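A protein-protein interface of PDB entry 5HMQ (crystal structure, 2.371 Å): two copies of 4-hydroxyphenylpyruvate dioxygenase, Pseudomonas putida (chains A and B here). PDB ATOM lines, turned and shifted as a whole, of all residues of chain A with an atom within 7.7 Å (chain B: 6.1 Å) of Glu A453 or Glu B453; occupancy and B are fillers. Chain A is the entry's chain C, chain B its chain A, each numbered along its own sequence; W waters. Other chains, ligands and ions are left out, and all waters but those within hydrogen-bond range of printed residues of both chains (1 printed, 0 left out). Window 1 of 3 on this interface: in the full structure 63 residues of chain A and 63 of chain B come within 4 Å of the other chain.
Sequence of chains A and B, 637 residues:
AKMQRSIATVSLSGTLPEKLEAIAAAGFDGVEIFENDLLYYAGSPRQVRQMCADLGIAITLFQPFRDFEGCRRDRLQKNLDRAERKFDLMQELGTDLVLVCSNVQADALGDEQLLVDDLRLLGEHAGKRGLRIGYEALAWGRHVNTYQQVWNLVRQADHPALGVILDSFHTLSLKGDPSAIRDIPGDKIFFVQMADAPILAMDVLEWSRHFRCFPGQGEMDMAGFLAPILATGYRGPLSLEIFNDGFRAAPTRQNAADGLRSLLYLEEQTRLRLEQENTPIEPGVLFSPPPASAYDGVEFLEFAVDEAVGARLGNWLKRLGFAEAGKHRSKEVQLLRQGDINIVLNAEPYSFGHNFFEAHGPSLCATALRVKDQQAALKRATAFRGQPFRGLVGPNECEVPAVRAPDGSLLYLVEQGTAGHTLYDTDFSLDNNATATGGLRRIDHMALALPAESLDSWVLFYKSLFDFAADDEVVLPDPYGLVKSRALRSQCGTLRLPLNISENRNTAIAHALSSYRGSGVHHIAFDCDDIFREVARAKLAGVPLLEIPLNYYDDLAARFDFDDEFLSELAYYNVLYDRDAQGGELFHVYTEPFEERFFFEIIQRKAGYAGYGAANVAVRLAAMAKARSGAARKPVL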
ATOM      1  N   PHE A 247     -30.025  18.247  -3.451  1.00  0.00           N
ATOM      2  CA  PHE A 247     -29.034  19.124  -2.849  1.00  0.00           C
ATOM      3  C   PHE A 247     -29.624  20.532  -2.731  1.00  0.00           C
ATOM      4  O   PHE A 247     -29.958  21.148  -3.746  1.00  0.00           O
ATOM      5  CB  PHE A 247     -27.751  19.169  -3.686  1.00  0.00           C
ATOM      6  CG  PHE A 247     -27.323  17.838  -4.251  1.00  0.00           C
ATOM      7  CD1 PHE A 247     -27.806  17.399  -5.475  1.00  0.00           C
ATOM      8  CD2 PHE A 247     -26.396  17.051  -3.583  1.00  0.00           C
ATOM      9  CE1 PHE A 247     -27.399  16.187  -6.007  1.00  0.00           C
ATOM     10  CE2 PHE A 247     -25.980  15.841  -4.112  1.00  0.00           C
ATOM     11  CZ  PHE A 247     -26.483  15.409  -5.325  1.00  0.00           C
ATOM     12  N   ARG A 248     -29.764  21.040  -1.509  1.00  0.00           N
ATOM     13  CA  ARG A 248     -29.413  20.315  -0.303  1.00  0.00           C
ATOM     14  C   ARG A 248     -29.754  21.083   0.965  1.00  0.00           C
ATOM     15  O   ARG A 248     -29.164  22.129   1.244  1.00  0.00           O
ATOM     16  N   ALA A 249     -30.711  20.564   1.733  1.00  0.00           N
ATOM     17  CA  ALA A 249     -31.070  21.158   3.008  1.00  0.00           C
ATOM     18  C   ALA A 249     -31.782  22.493   2.904  1.00  0.00           C
ATOM     19  O   ALA A 249     -31.383  23.471   3.545  1.00  0.00           O
ATOM     20  N   ALA A 250     -32.834  22.541   2.097  1.00  0.00           N
ATOM     21  CA  ALA A 250     -33.662  23.735   1.937  1.00  0.00           C
ATOM     22  C   ALA A 250     -34.674  23.820   3.076  1.00  0.00           C
ATOM     23  O   ALA A 250     -35.410  22.855   3.312  1.00  0.00           O
ATOM     24  CB  ALA A 250     -34.379  23.723   0.590  1.00  0.00           C
ATOM     25  N   PRO A 251     -34.735  24.941   3.812  1.00  0.00           N
ATOM     26  CA  PRO A 251     -35.676  25.021   4.939  1.00  0.00           C
ATOM     27  C   PRO A 251     -37.122  24.891   4.487  1.00  0.00           C
ATOM     28  O   PRO A 251     -37.655  25.746   3.773  1.00  0.00           O
ATOM     29  CB  PRO A 251     -35.398  26.406   5.536  1.00  0.00           C
ATOM     30  CG  PRO A 251     -34.806  27.194   4.415  1.00  0.00           C
ATOM     31  CD  PRO A 251     -34.042  26.217   3.566  1.00  0.00           C
ATOM     32  N   ASN A 255     -39.458  28.047   3.142  1.00  0.00           N
ATOM     33  CA  ASN A 255     -39.760  27.961   1.717  1.00  0.00           C
ATOM     34  C   ASN A 255     -41.265  27.950   1.481  1.00  0.00           C
ATOM     35  O   ASN A 255     -41.761  28.612   0.562  1.00  0.00           O
ATOM     36  CB  ASN A 255     -39.107  26.724   1.102  1.00  0.00           C
ATOM     37  CG  ASN A 255     -37.631  26.922   0.814  1.00  0.00           C
ATOM     38  OD1 ASN A 255     -37.115  28.037   0.888  1.00  0.00           O
ATOM     39  ND2 ASN A 255     -36.946  25.839   0.463  1.00  0.00           N
ATOM     40  N   ASP A 258     -42.534  31.477   2.198  1.00  0.00           N
ATOM     41  CA  ASP A 258     -42.168  32.340   1.078  1.00  0.00           C
ATOM     42  C   ASP A 258     -43.053  32.074  -0.132  1.00  0.00           C
ATOM     43  O   ASP A 258     -43.450  33.008  -0.839  1.00  0.00           O
ATOM     44  CB  ASP A 258     -40.696  32.139   0.712  1.00  0.00           C
ATOM     45  CG  ASP A 258     -39.749  32.791   1.703  1.00  0.00           C
ATOM     46  OD1 ASP A 258     -40.214  33.587   2.544  1.00  0.00           O
ATOM     47  OD2 ASP A 258     -38.533  32.510   1.633  1.00  0.00           O
ATOM     48  N   LEU A 450     -25.436  39.120   2.031  1.00  0.00           N
ATOM     49  CA  LEU A 450     -26.347  38.083   2.488  1.00  0.00           C
ATOM     50  C   LEU A 450     -25.888  36.708   2.019  1.00  0.00           C
ATOM     51  O   LEU A 450     -25.215  36.594   0.990  1.00  0.00           O
ATOM     52  CB  LEU A 450     -27.771  38.339   1.974  1.00  0.00           C
ATOM     53  CG  LEU A 450     -28.438  39.647   2.409  1.00  0.00           C
ATOM     54  CD1 LEU A 450     -29.750  39.856   1.665  1.00  0.00           C
ATOM     55  CD2 LEU A 450     -28.664  39.659   3.912  1.00  0.00           C
ATOM     56  N   PRO A 451     -26.227  35.647   2.755  1.00  0.00           N
ATOM     57  CA  PRO A 451     -25.931  34.296   2.265  1.00  0.00           C
ATOM     58  C   PRO A 451     -26.667  34.026   0.963  1.00  0.00           C
ATOM     59  O   PRO A 451     -27.799  34.471   0.765  1.00  0.00           O
ATOM     60  CB  PRO A 451     -26.428  33.386   3.395  1.00  0.00           C
ATOM     61  CG  PRO A 451     -26.498  34.262   4.598  1.00  0.00           C
ATOM     62  CD  PRO A 451     -26.853  35.626   4.087  1.00  0.00           C
ATOM     63  N   ALA A 452     -25.999  33.299   0.065  1.00  0.00           N
ATOM     64  CA  ALA A 452     -26.566  33.029  -1.253  1.00  0.00           C
ATOM     65  C   ALA A 452     -27.926  32.345  -1.155  1.00  0.00           C
ATOM     66  O   ALA A 452     -28.822  32.612  -1.963  1.00  0.00           O
ATOM     67  CB  ALA A 452     -25.596  32.179  -2.074  1.00  0.00           C
ATOM     68  N   GLU A 453     -28.099  31.456  -0.178  1.00  0.00           N
ATOM     69  CA  GLU A 453     -29.325  30.674  -0.074  1.00  0.00           C
ATOM     70  C   GLU A 453     -30.493  31.458   0.507  1.00  0.00           C
ATOM     71  O   GLU A 453     -31.632  30.985   0.423  1.00  0.00           O
ATOM     72  CB  GLU A 453     -29.099  29.428   0.792  1.00  0.00           C
ATOM     73  CG  GLU A 453     -27.726  28.790   0.654  1.00  0.00           C
ATOM     74  CD  GLU A 453     -26.665  29.544   1.443  1.00  0.00           C
ATOM     75  OE1 GLU A 453     -27.023  30.161   2.469  1.00  0.00           O
ATOM     76  OE2 GLU A 453     -25.491  29.554   1.025  1.00  0.00           O
ATOM     77  N   SER A 454     -30.252  32.632   1.090  1.00  0.00           N
ATOM     78  CA  SER A 454     -31.316  33.411   1.719  1.00  0.00           C
ATOM     79  C   SER A 454     -31.648  34.690   0.961  1.00  0.00           C
ATOM     80  O   SER A 454     -32.566  35.407   1.364  1.00  0.00           O
ATOM     81  CB  SER A 454     -30.945  33.747   3.168  1.00  0.00           C
ATOM     82  OG  SER A 454     -29.726  34.460   3.237  1.00  0.00           O
ATOM     83  N   LEU A 455     -30.931  34.984  -0.133  1.00  0.00           N
ATOM     84  CA  LEU A 455     -31.083  36.275  -0.793  1.00  0.00           C
ATOM     85  C   LEU A 455     -32.446  36.418  -1.456  1.00  0.00           C
ATOM     86  O   LEU A 455     -33.084  37.472  -1.356  1.00  0.00           O
ATOM     87  CB  LEU A 455     -29.981  36.475  -1.841  1.00  0.00           C
ATOM     88  CG  LEU A 455     -30.137  37.674  -2.783  1.00  0.00           C
ATOM     89  CD1 LEU A 455     -29.851  39.006  -2.099  1.00  0.00           C
ATOM     90  CD2 LEU A 455     -29.216  37.468  -3.975  1.00  0.00           C
ATOM     91  N   ASP A 456     -32.920  35.367  -2.121  1.00  0.00           N
ATOM     92  CA  ASP A 456     -34.238  35.426  -2.750  1.00  0.00           C
ATOM     93  C   ASP A 456     -35.330  35.670  -1.721  1.00  0.00           C
ATOM     94  O   ASP A 456     -36.308  36.368  -2.003  1.00  0.00           O
ATOM     95  CB  ASP A 456     -34.511  34.142  -3.549  1.00  0.00           C
ATOM     96  CG  ASP A 456     -33.664  34.057  -4.807  1.00  0.00           C
ATOM     97  OD1 ASP A 456     -33.195  35.113  -5.286  1.00  0.00           O
ATOM     98  OD2 ASP A 456     -33.498  32.939  -5.340  1.00  0.00           O
ATOM     99  N   SER A 457     -35.183  35.100  -0.523  1.00  0.00           N
ATOM    100  CA  SER A 457     -36.159  35.349   0.533  1.00  0.00           C
ATOM    101  C   SER A 457     -36.145  36.814   0.957  1.00  0.00           C
ATOM    102  O   SER A 457     -37.204  37.414   1.181  1.00  0.00           O
ATOM    103  CB  SER A 457     -35.878  34.439   1.727  1.00  0.00           C
ATOM    104  OG  SER A 457     -36.946  34.469   2.651  1.00  0.00           O
ATOM    105  N   TRP A 458     -34.953  37.410   1.067  1.00  0.00           N
ATOM    106  CA  TRP A 458     -34.865  38.835   1.380  1.00  0.00           C
ATOM    107  C   TRP A 458     -35.457  39.685   0.263  1.00  0.00           C
ATOM    108  O   TRP A 458     -36.109  40.703   0.526  1.00  0.00           O
ATOM    109  CB  TRP A 458     -33.413  39.238   1.637  1.00  0.00           C
ATOM    110  CG  TRP A 458     -32.922  38.957   3.023  1.00  0.00           C
ATOM    111  CD1 TRP A 458     -32.498  37.760   3.515  1.00  0.00           C
ATOM    112  CD2 TRP A 458     -32.788  39.903   4.094  1.00  0.00           C
ATOM    113  NE1 TRP A 458     -32.113  37.897   4.828  1.00  0.00           N
ATOM    114  CE2 TRP A 458     -32.281  39.203   5.206  1.00  0.00           C
ATOM    115  CE3 TRP A 458     -33.050  41.271   4.219  1.00  0.00           C
ATOM    116  CZ2 TRP A 458     -32.032  39.825   6.429  1.00  0.00           C
ATOM    117  CZ3 TRP A 458     -32.801  41.887   5.433  1.00  0.00           C
ATOM    118  CH2 TRP A 458     -32.298  41.164   6.522  1.00  0.00           C
ATOM    119  N   ILE A 501     -23.432  38.954  -2.011  1.00  0.00           N
ATOM    120  CA  ILE A 501     -23.393  37.579  -1.528  1.00  0.00           C
ATOM    121  C   ILE A 501     -22.246  37.446  -0.537  1.00  0.00           C
ATOM    122  O   ILE A 501     -21.087  37.719  -0.872  1.00  0.00           O
ATOM    123  CB  ILE A 501     -23.247  36.582  -2.687  1.00  0.00           C
ATOM    124  CG1 ILE A 501     -24.454  36.686  -3.621  1.00  0.00           C
ATOM    125  CG2 ILE A 501     -23.094  35.167  -2.152  1.00  0.00           C
ATOM    126  CD1 ILE A 501     -24.370  35.791  -4.838  1.00  0.00           C
ATOM    127  N   SER A 502     -22.573  37.046   0.690  1.00  0.00           N
ATOM    128  CA  SER A 502     -21.556  36.789   1.696  1.00  0.00           C
ATOM    129  C   SER A 502     -20.802  35.503   1.389  1.00  0.00           C
ATOM    130  O   SER A 502     -21.261  34.636   0.640  1.00  0.00           O
ATOM    131  CB  SER A 502     -22.184  36.669   3.087  1.00  0.00           C
ATOM    132  OG  SER A 502     -22.821  37.867   3.474  1.00  0.00           O
ATOM    133  N   GLU A 503     -19.618  35.394   1.981  1.00  0.00           N
ATOM    134  CA  GLU A 503     -18.806  34.197   1.843  1.00  0.00           C
ATOM    135  C   GLU A 503     -19.337  33.132   2.794  1.00  0.00           C
ATOM    136  O   GLU A 503     -19.759  33.438   3.911  1.00  0.00           O
ATOM    137  CB  GLU A 503     -17.341  34.513   2.150  1.00  0.00           C
ATOM    138  CG  GLU A 503     -16.362  33.450   1.695  1.00  0.00           C
ATOM    139  CD  GLU A 503     -16.405  33.235   0.196  1.00  0.00           C
ATOM    140  OE1 GLU A 503     -17.136  32.327  -0.253  1.00  0.00           O
ATOM    141  OE2 GLU A 503     -15.718  33.985  -0.533  1.00  0.00           O
ATOM    142  N   ASN A 504     -19.340  31.880   2.344  1.00  0.00           N
ATOM    143  CA  ASN A 504     -19.798  30.802   3.203  1.00  0.00           C
ATOM    144  C   ASN A 504     -18.789  30.580   4.322  1.00  0.00           C
ATOM    145  O   ASN A 504     -17.649  31.045   4.266  1.00  0.00           O
ATOM    146  CB  ASN A 504     -19.994  29.494   2.428  1.00  0.00           C
ATOM    147  CG  ASN A 504     -18.683  28.827   2.015  1.00  0.00           C
ATOM    148  OD1 ASN A 504     -17.758  28.748   2.803  1.00  0.00           O
ATOM    149  ND2 ASN A 504     -18.621  28.313   0.793  1.00  0.00           N
ATOM    150  N   ARG A 505     -19.234  29.922   5.390  1.00  0.00           N
ATOM    151  CA  ARG A 505     -18.282  29.574   6.440  1.00  0.00           C
ATOM    152  C   ARG A 505     -17.305  28.495   5.969  1.00  0.00           C
ATOM    153  O   ARG A 505     -16.123  28.529   6.323  1.00  0.00           O
ATOM    154  CB  ARG A 505     -19.016  29.143   7.708  1.00  0.00           C
ATOM    155  CG  ARG A 505     -20.069  28.071   7.527  1.00  0.00           C
ATOM    156  CD  ARG A 505     -20.729  27.765   8.864  1.00  0.00           C
ATOM    157  NE  ARG A 505     -21.308  26.426   8.901  1.00  0.00           N
ATOM    158  CZ  ARG A 505     -21.581  25.760  10.020  1.00  0.00           C
ATOM    159  NH1 ARG A 505     -21.322  26.305  11.201  1.00  0.00           N
ATOM    160  NH2 ARG A 505     -22.107  24.543   9.960  1.00  0.00           N
ATOM    161  N   ASN A 506     -17.778  27.536   5.160  1.00  0.00           N
ATOM    162  CA  ASN A 506     -16.950  26.397   4.753  1.00  0.00           C
ATOM    163  C   ASN A 506     -15.816  26.762   3.791  1.00  0.00           C
ATOM    164  O   ASN A 506     -14.848  26.000   3.681  1.00  0.00           O
ATOM    165  CB  ASN A 506     -17.834  25.317   4.124  1.00  0.00           C
ATOM    166  CG  ASN A 506     -18.449  24.389   5.163  1.00  0.00           C
ATOM    167  OD1 ASN A 506     -18.275  24.584   6.366  1.00  0.00           O
ATOM    168  ND2 ASN A 506     -19.178  23.380   4.702  1.00  0.00           N
ATOM    169  N   PHE B 247     -29.058  34.663   9.679  1.00  0.00           N
ATOM    170  CA  PHE B 247     -29.176  34.865   8.235  1.00  0.00           C
ATOM    171  C   PHE B 247     -29.643  33.582   7.543  1.00  0.00           C
ATOM    172  O   PHE B 247     -28.916  32.917   6.800  1.00  0.00           O
ATOM    173  CB  PHE B 247     -27.863  35.384   7.674  1.00  0.00           C
ATOM    174  CG  PHE B 247     -27.628  36.833   7.973  1.00  0.00           C
ATOM    175  CD1 PHE B 247     -28.160  37.814   7.154  1.00  0.00           C
ATOM    176  CD2 PHE B 247     -26.910  37.218   9.093  1.00  0.00           C
ATOM    177  CE1 PHE B 247     -27.960  39.151   7.432  1.00  0.00           C
ATOM    178  CE2 PHE B 247     -26.708  38.554   9.378  1.00  0.00           C
ATOM    179  CZ  PHE B 247     -27.234  39.523   8.546  1.00  0.00           C
ATOM    180  N   ALA B 249     -31.703  30.177   6.004  1.00  0.00           N
ATOM    181  CA  ALA B 249     -31.383  28.780   5.743  1.00  0.00           C
ATOM    182  C   ALA B 249     -31.517  27.956   7.015  1.00  0.00           C
ATOM    183  O   ALA B 249     -32.394  28.223   7.843  1.00  0.00           O
ATOM    184  CB  ALA B 249     -29.978  28.638   5.154  1.00  0.00           C
ATOM    185  N   LEU B 450     -20.718  18.952  -3.255  1.00  0.00           N
ATOM    186  CA  LEU B 450     -21.890  19.137  -2.422  1.00  0.00           C
ATOM    187  C   LEU B 450     -22.083  20.611  -2.092  1.00  0.00           C
ATOM    188  O   LEU B 450     -21.115  21.378  -2.072  1.00  0.00           O
ATOM    189  CB  LEU B 450     -21.764  18.339  -1.117  1.00  0.00           C
ATOM    190  CG  LEU B 450     -21.615  16.823  -1.262  1.00  0.00           C
ATOM    191  CD1 LEU B 450     -21.305  16.187   0.085  1.00  0.00           C
ATOM    192  CD2 LEU B 450     -22.862  16.213  -1.879  1.00  0.00           C
ATOM    193  N   PRO B 451     -23.319  21.042  -1.845  1.00  0.00           N
ATOM    194  CA  PRO B 451     -23.535  22.421  -1.391  1.00  0.00           C
ATOM    195  C   PRO B 451     -22.842  22.667  -0.060  1.00  0.00           C
ATOM    196  O   PRO B 451     -22.796  21.792   0.807  1.00  0.00           O
ATOM    197  CB  PRO B 451     -25.059  22.523  -1.265  1.00  0.00           C
ATOM    198  CG  PRO B 451     -25.590  21.420  -2.113  1.00  0.00           C
ATOM    199  CD  PRO B 451     -24.588  20.316  -2.028  1.00  0.00           C
ATOM    200  N   ALA B 452     -22.294  23.875   0.087  1.00  0.00           N
ATOM    201  CA  ALA B 452     -21.536  24.216   1.288  1.00  0.00           C
ATOM    202  C   ALA B 452     -22.364  24.006   2.550  1.00  0.00           C
ATOM    203  O   ALA B 452     -21.837  23.573   3.581  1.00  0.00           O
ATOM    204  CB  ALA B 452     -21.046  25.661   1.202  1.00  0.00           C
ATOM    205  N   GLU B 453     -23.660  24.312   2.489  1.00  0.00           N
ATOM    206  CA  GLU B 453     -24.533  24.233   3.653  1.00  0.00           C
ATOM    207  C   GLU B 453     -24.962  22.809   3.985  1.00  0.00           C
ATOM    208  O   GLU B 453     -25.520  22.586   5.065  1.00  0.00           O
ATOM    209  CB  GLU B 453     -25.783  25.097   3.447  1.00  0.00           C
ATOM    210  CG  GLU B 453     -25.540  26.421   2.732  1.00  0.00           C
ATOM    211  CD  GLU B 453     -25.376  26.266   1.222  1.00  0.00           C
ATOM    212  OE1 GLU B 453     -24.625  27.055   0.618  1.00  0.00           O
ATOM    213  OE2 GLU B 453     -25.970  25.330   0.655  1.00  0.00           O
ATOM    214  N   SER B 454     -24.713  21.845   3.100  1.00  0.00           N
ATOM    215  CA  SER B 454     -25.139  20.470   3.310  1.00  0.00           C
ATOM    216  C   SER B 454     -23.984  19.524   3.592  1.00  0.00           C
ATOM    217  O   SER B 454     -24.221  18.351   3.886  1.00  0.00           O
ATOM    218  CB  SER B 454     -25.909  19.964   2.089  1.00  0.00           C
ATOM    219  OG  SER B 454     -26.819  20.941   1.622  1.00  0.00           O
ATOM    220  N   LEU B 455     -22.743  20.000   3.524  1.00  0.00           N
ATOM    221  CA  LEU B 455     -21.601  19.092   3.585  1.00  0.00           C
ATOM    222  C   LEU B 455     -21.425  18.514   4.987  1.00  0.00           C
ATOM    223  O   LEU B 455     -21.108  17.329   5.137  1.00  0.00           O
ATOM    224  CB  LEU B 455     -20.340  19.817   3.106  1.00  0.00           C
ATOM    225  CG  LEU B 455     -19.014  19.068   3.096  1.00  0.00           C
ATOM    226  CD1 LEU B 455     -18.223  19.509   1.863  1.00  0.00           C
ATOM    227  CD2 LEU B 455     -18.213  19.359   4.358  1.00  0.00           C
ATOM    228  N   ASP B 456     -21.629  19.332   6.025  1.00  0.00           N
ATOM    229  CA  ASP B 456     -21.515  18.829   7.390  1.00  0.00           C
ATOM    230  C   ASP B 456     -22.518  17.712   7.652  1.00  0.00           C
ATOM    231  O   ASP B 456     -22.213  16.746   8.364  1.00  0.00           O
ATOM    232  CB  ASP B 456     -21.702  19.969   8.390  1.00  0.00           C
ATOM    233  CG  ASP B 456     -20.544  20.950   8.380  1.00  0.00           C
ATOM    234  OD1 ASP B 456     -19.442  20.564   7.936  1.00  0.00           O
ATOM    235  OD2 ASP B 456     -20.737  22.108   8.809  1.00  0.00           O
ATOM    236  N   SER B 457     -23.722  17.826   7.085  1.00  0.00           N
ATOM    237  CA  SER B 457     -24.718  16.770   7.233  1.00  0.00           C
ATOM    238  C   SER B 457     -24.268  15.486   6.544  1.00  0.00           C
ATOM    239  O   SER B 457     -24.481  14.387   7.070  1.00  0.00           O
ATOM    240  CB  SER B 457     -26.065  17.238   6.681  1.00  0.00           C
ATOM    241  OG  SER B 457     -27.103  16.343   7.042  1.00  0.00           O
ATOM    242  N   ASN B 504     -22.780  27.591  -5.725  1.00  0.00           N
ATOM    243  CA  ASN B 504     -24.193  27.894  -5.543  1.00  0.00           C
ATOM    244  C   ASN B 504     -24.731  28.498  -6.837  1.00  0.00           C
ATOM    245  O   ASN B 504     -23.984  29.092  -7.624  1.00  0.00           O
ATOM    246  CB  ASN B 504     -24.399  28.798  -4.327  1.00  0.00           C
ATOM    247  CG  ASN B 504     -23.675  30.124  -4.439  1.00  0.00           C
ATOM    248  OD1 ASN B 504     -23.705  30.784  -5.468  1.00  0.00           O
ATOM    249  ND2 ASN B 504     -23.003  30.513  -3.361  1.00  0.00           N
ATOM    250  N   ASN B 506     -26.685  31.045  -7.287  1.00  0.00           N
ATOM    251  CA  ASN B 506     -26.716  32.502  -7.311  1.00  0.00           C
ATOM    252  C   ASN B 506     -25.387  33.116  -7.739  1.00  0.00           C
ATOM    253  O   ASN B 506     -25.360  34.290  -8.122  1.00  0.00           O
ATOM    254  CB  ASN B 506     -27.135  33.023  -5.934  1.00  0.00           C
ATOM    255  CG  ASN B 506     -28.645  33.079  -5.769  1.00  0.00           C
ATOM    256  OD1 ASN B 506     -29.374  33.373  -6.719  1.00  0.00           O
ATOM    257  ND2 ASN B 506     -29.124  32.769  -4.571  1.00  0.00           N
HETATM  258  O   HOH W   1     -22.164  22.407   6.229  1.00  0.00           O
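OE1 of Glu B453 sits close to OE2 of Glu A453, 2.7 Å away.
O of Ala B452 lies within hydrogen-bond range of ND2 of Asn A506.
ND2 of Asn B506 lies within hydrogen-bond range of O of Ala A452.
The side-chain carboxylate of Asp B456 lies within salt-bridge range of the guanidinium group of Arg A505.
The side-chain hydroxyl (OG) of Ser B454 sits at hydrogen-bond distance from the backbone carbonyl oxygen (O) of Arg A248.
O of Pro A251 lies close to ND2 of Asn A255 (3.4 Å).
The backbone carbonyl oxygen of Pro A451 lies within hydrogen-bond range of the side-chain hydroxyl of Ser A454 (3.1 Å).
The side-chain amide oxygen (OD1) of Asn A504 is in hydrogen-bond range of the backbone NH (N) of Asn A506 (2.7 Å).
O of Leu A450 sits at hydrogen-bond distance from N of Ser A502 (2.7 Å).
Among the printed residues, pairs that only touch across the chains: Ala A452 with Asn B504 (3.3 Å), Phe A247 with Pro B451 (3.5 Å), Pro A451 with Phe B247 (3.5 Å), Asn A504 with Ala B452 (3.6 Å), Leu A450 with Phe B247 (3.6 Å), Ile A501 with Asn B506 (3.7 Å), Phe A247 with Leu B450 (3.9 Å), Ala A249 with Ser B454 (3.9 Å), Ser A454 with Phe B247 (3.97 Å) and Pro A251 with Ala B249 (3.999 Å).
Ala A250 touches none of the printed residues of chain B.
Glu A453 touches just one residue of chain B: Glu B453.
Asp A456 touches none of the printed residues of chain B.
Of the printed residues of chain B, Ile A501 touches Asn B506 (3.7 Å).
Printed residues of chain B within 4 Å of Asn A506: Ala B452 (2.9 Å).
Printed residues of chain A within 4 Å of Leu B450: Phe A247.
Of chain A, only Asn A504 and Asn A506 come within 4 Å of Ala B452.
Glu B453 touches just one residue of chain A: Glu A453 (2.7 Å).
Of the printed residues of chain A, Ser B454 touches Arg A248 (2.7 Å) and Ala A249 (3.9 Å).
The nearest residue of chain B that does not touch Glu A453 is Ala B249 (4.3 Å).
Printed residues of chain B that touch a printed residue of chain A: Phe B247, Ala B249, Leu B450, Pro B451, Ala B452, Glu B453, Ser B454, Asp B456, Asn B504 and Asn B506.
Hydrophobic or aromatic side chains of chain B within 4 Å of the printed part of chain A: Phe B247, Leu B450, Pro B451 and Ala B452.
Of the 22 printed residues of chain A, 13 touch a printed residue of chain B.
Hydrophobic or aromatic side chains of chain A within 4 Å of the printed part of chain B: Phe A247, Pro A251, Leu A450, Pro A451, Ala A452 and Ile A501.
Among the printed residues, 15 pairs touch across the chains.
Phe A247 touches Leu B450, and with the chains exchanged Leu A450 touches Phe B247.
Phe A247 touches Pro B451, and with the chains exchanged Pro A451 touches Phe B247.
Ala A452 touches Asn B504, and with the chains exchanged Asn A504 touches Ala B452.
Glu A453 touches its own counterpart, Glu B453.
Of the 15 pairs that touch across the chains among the printed residues, 9 have their exchanged pair printed and touching as well.
Water W1 lies within hydrogen-bond range of O of Ala B452 (2.9 Å), OD2 of Asp B456 (3.0 Å) and ND2 of Asn A506 (3.5 Å).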
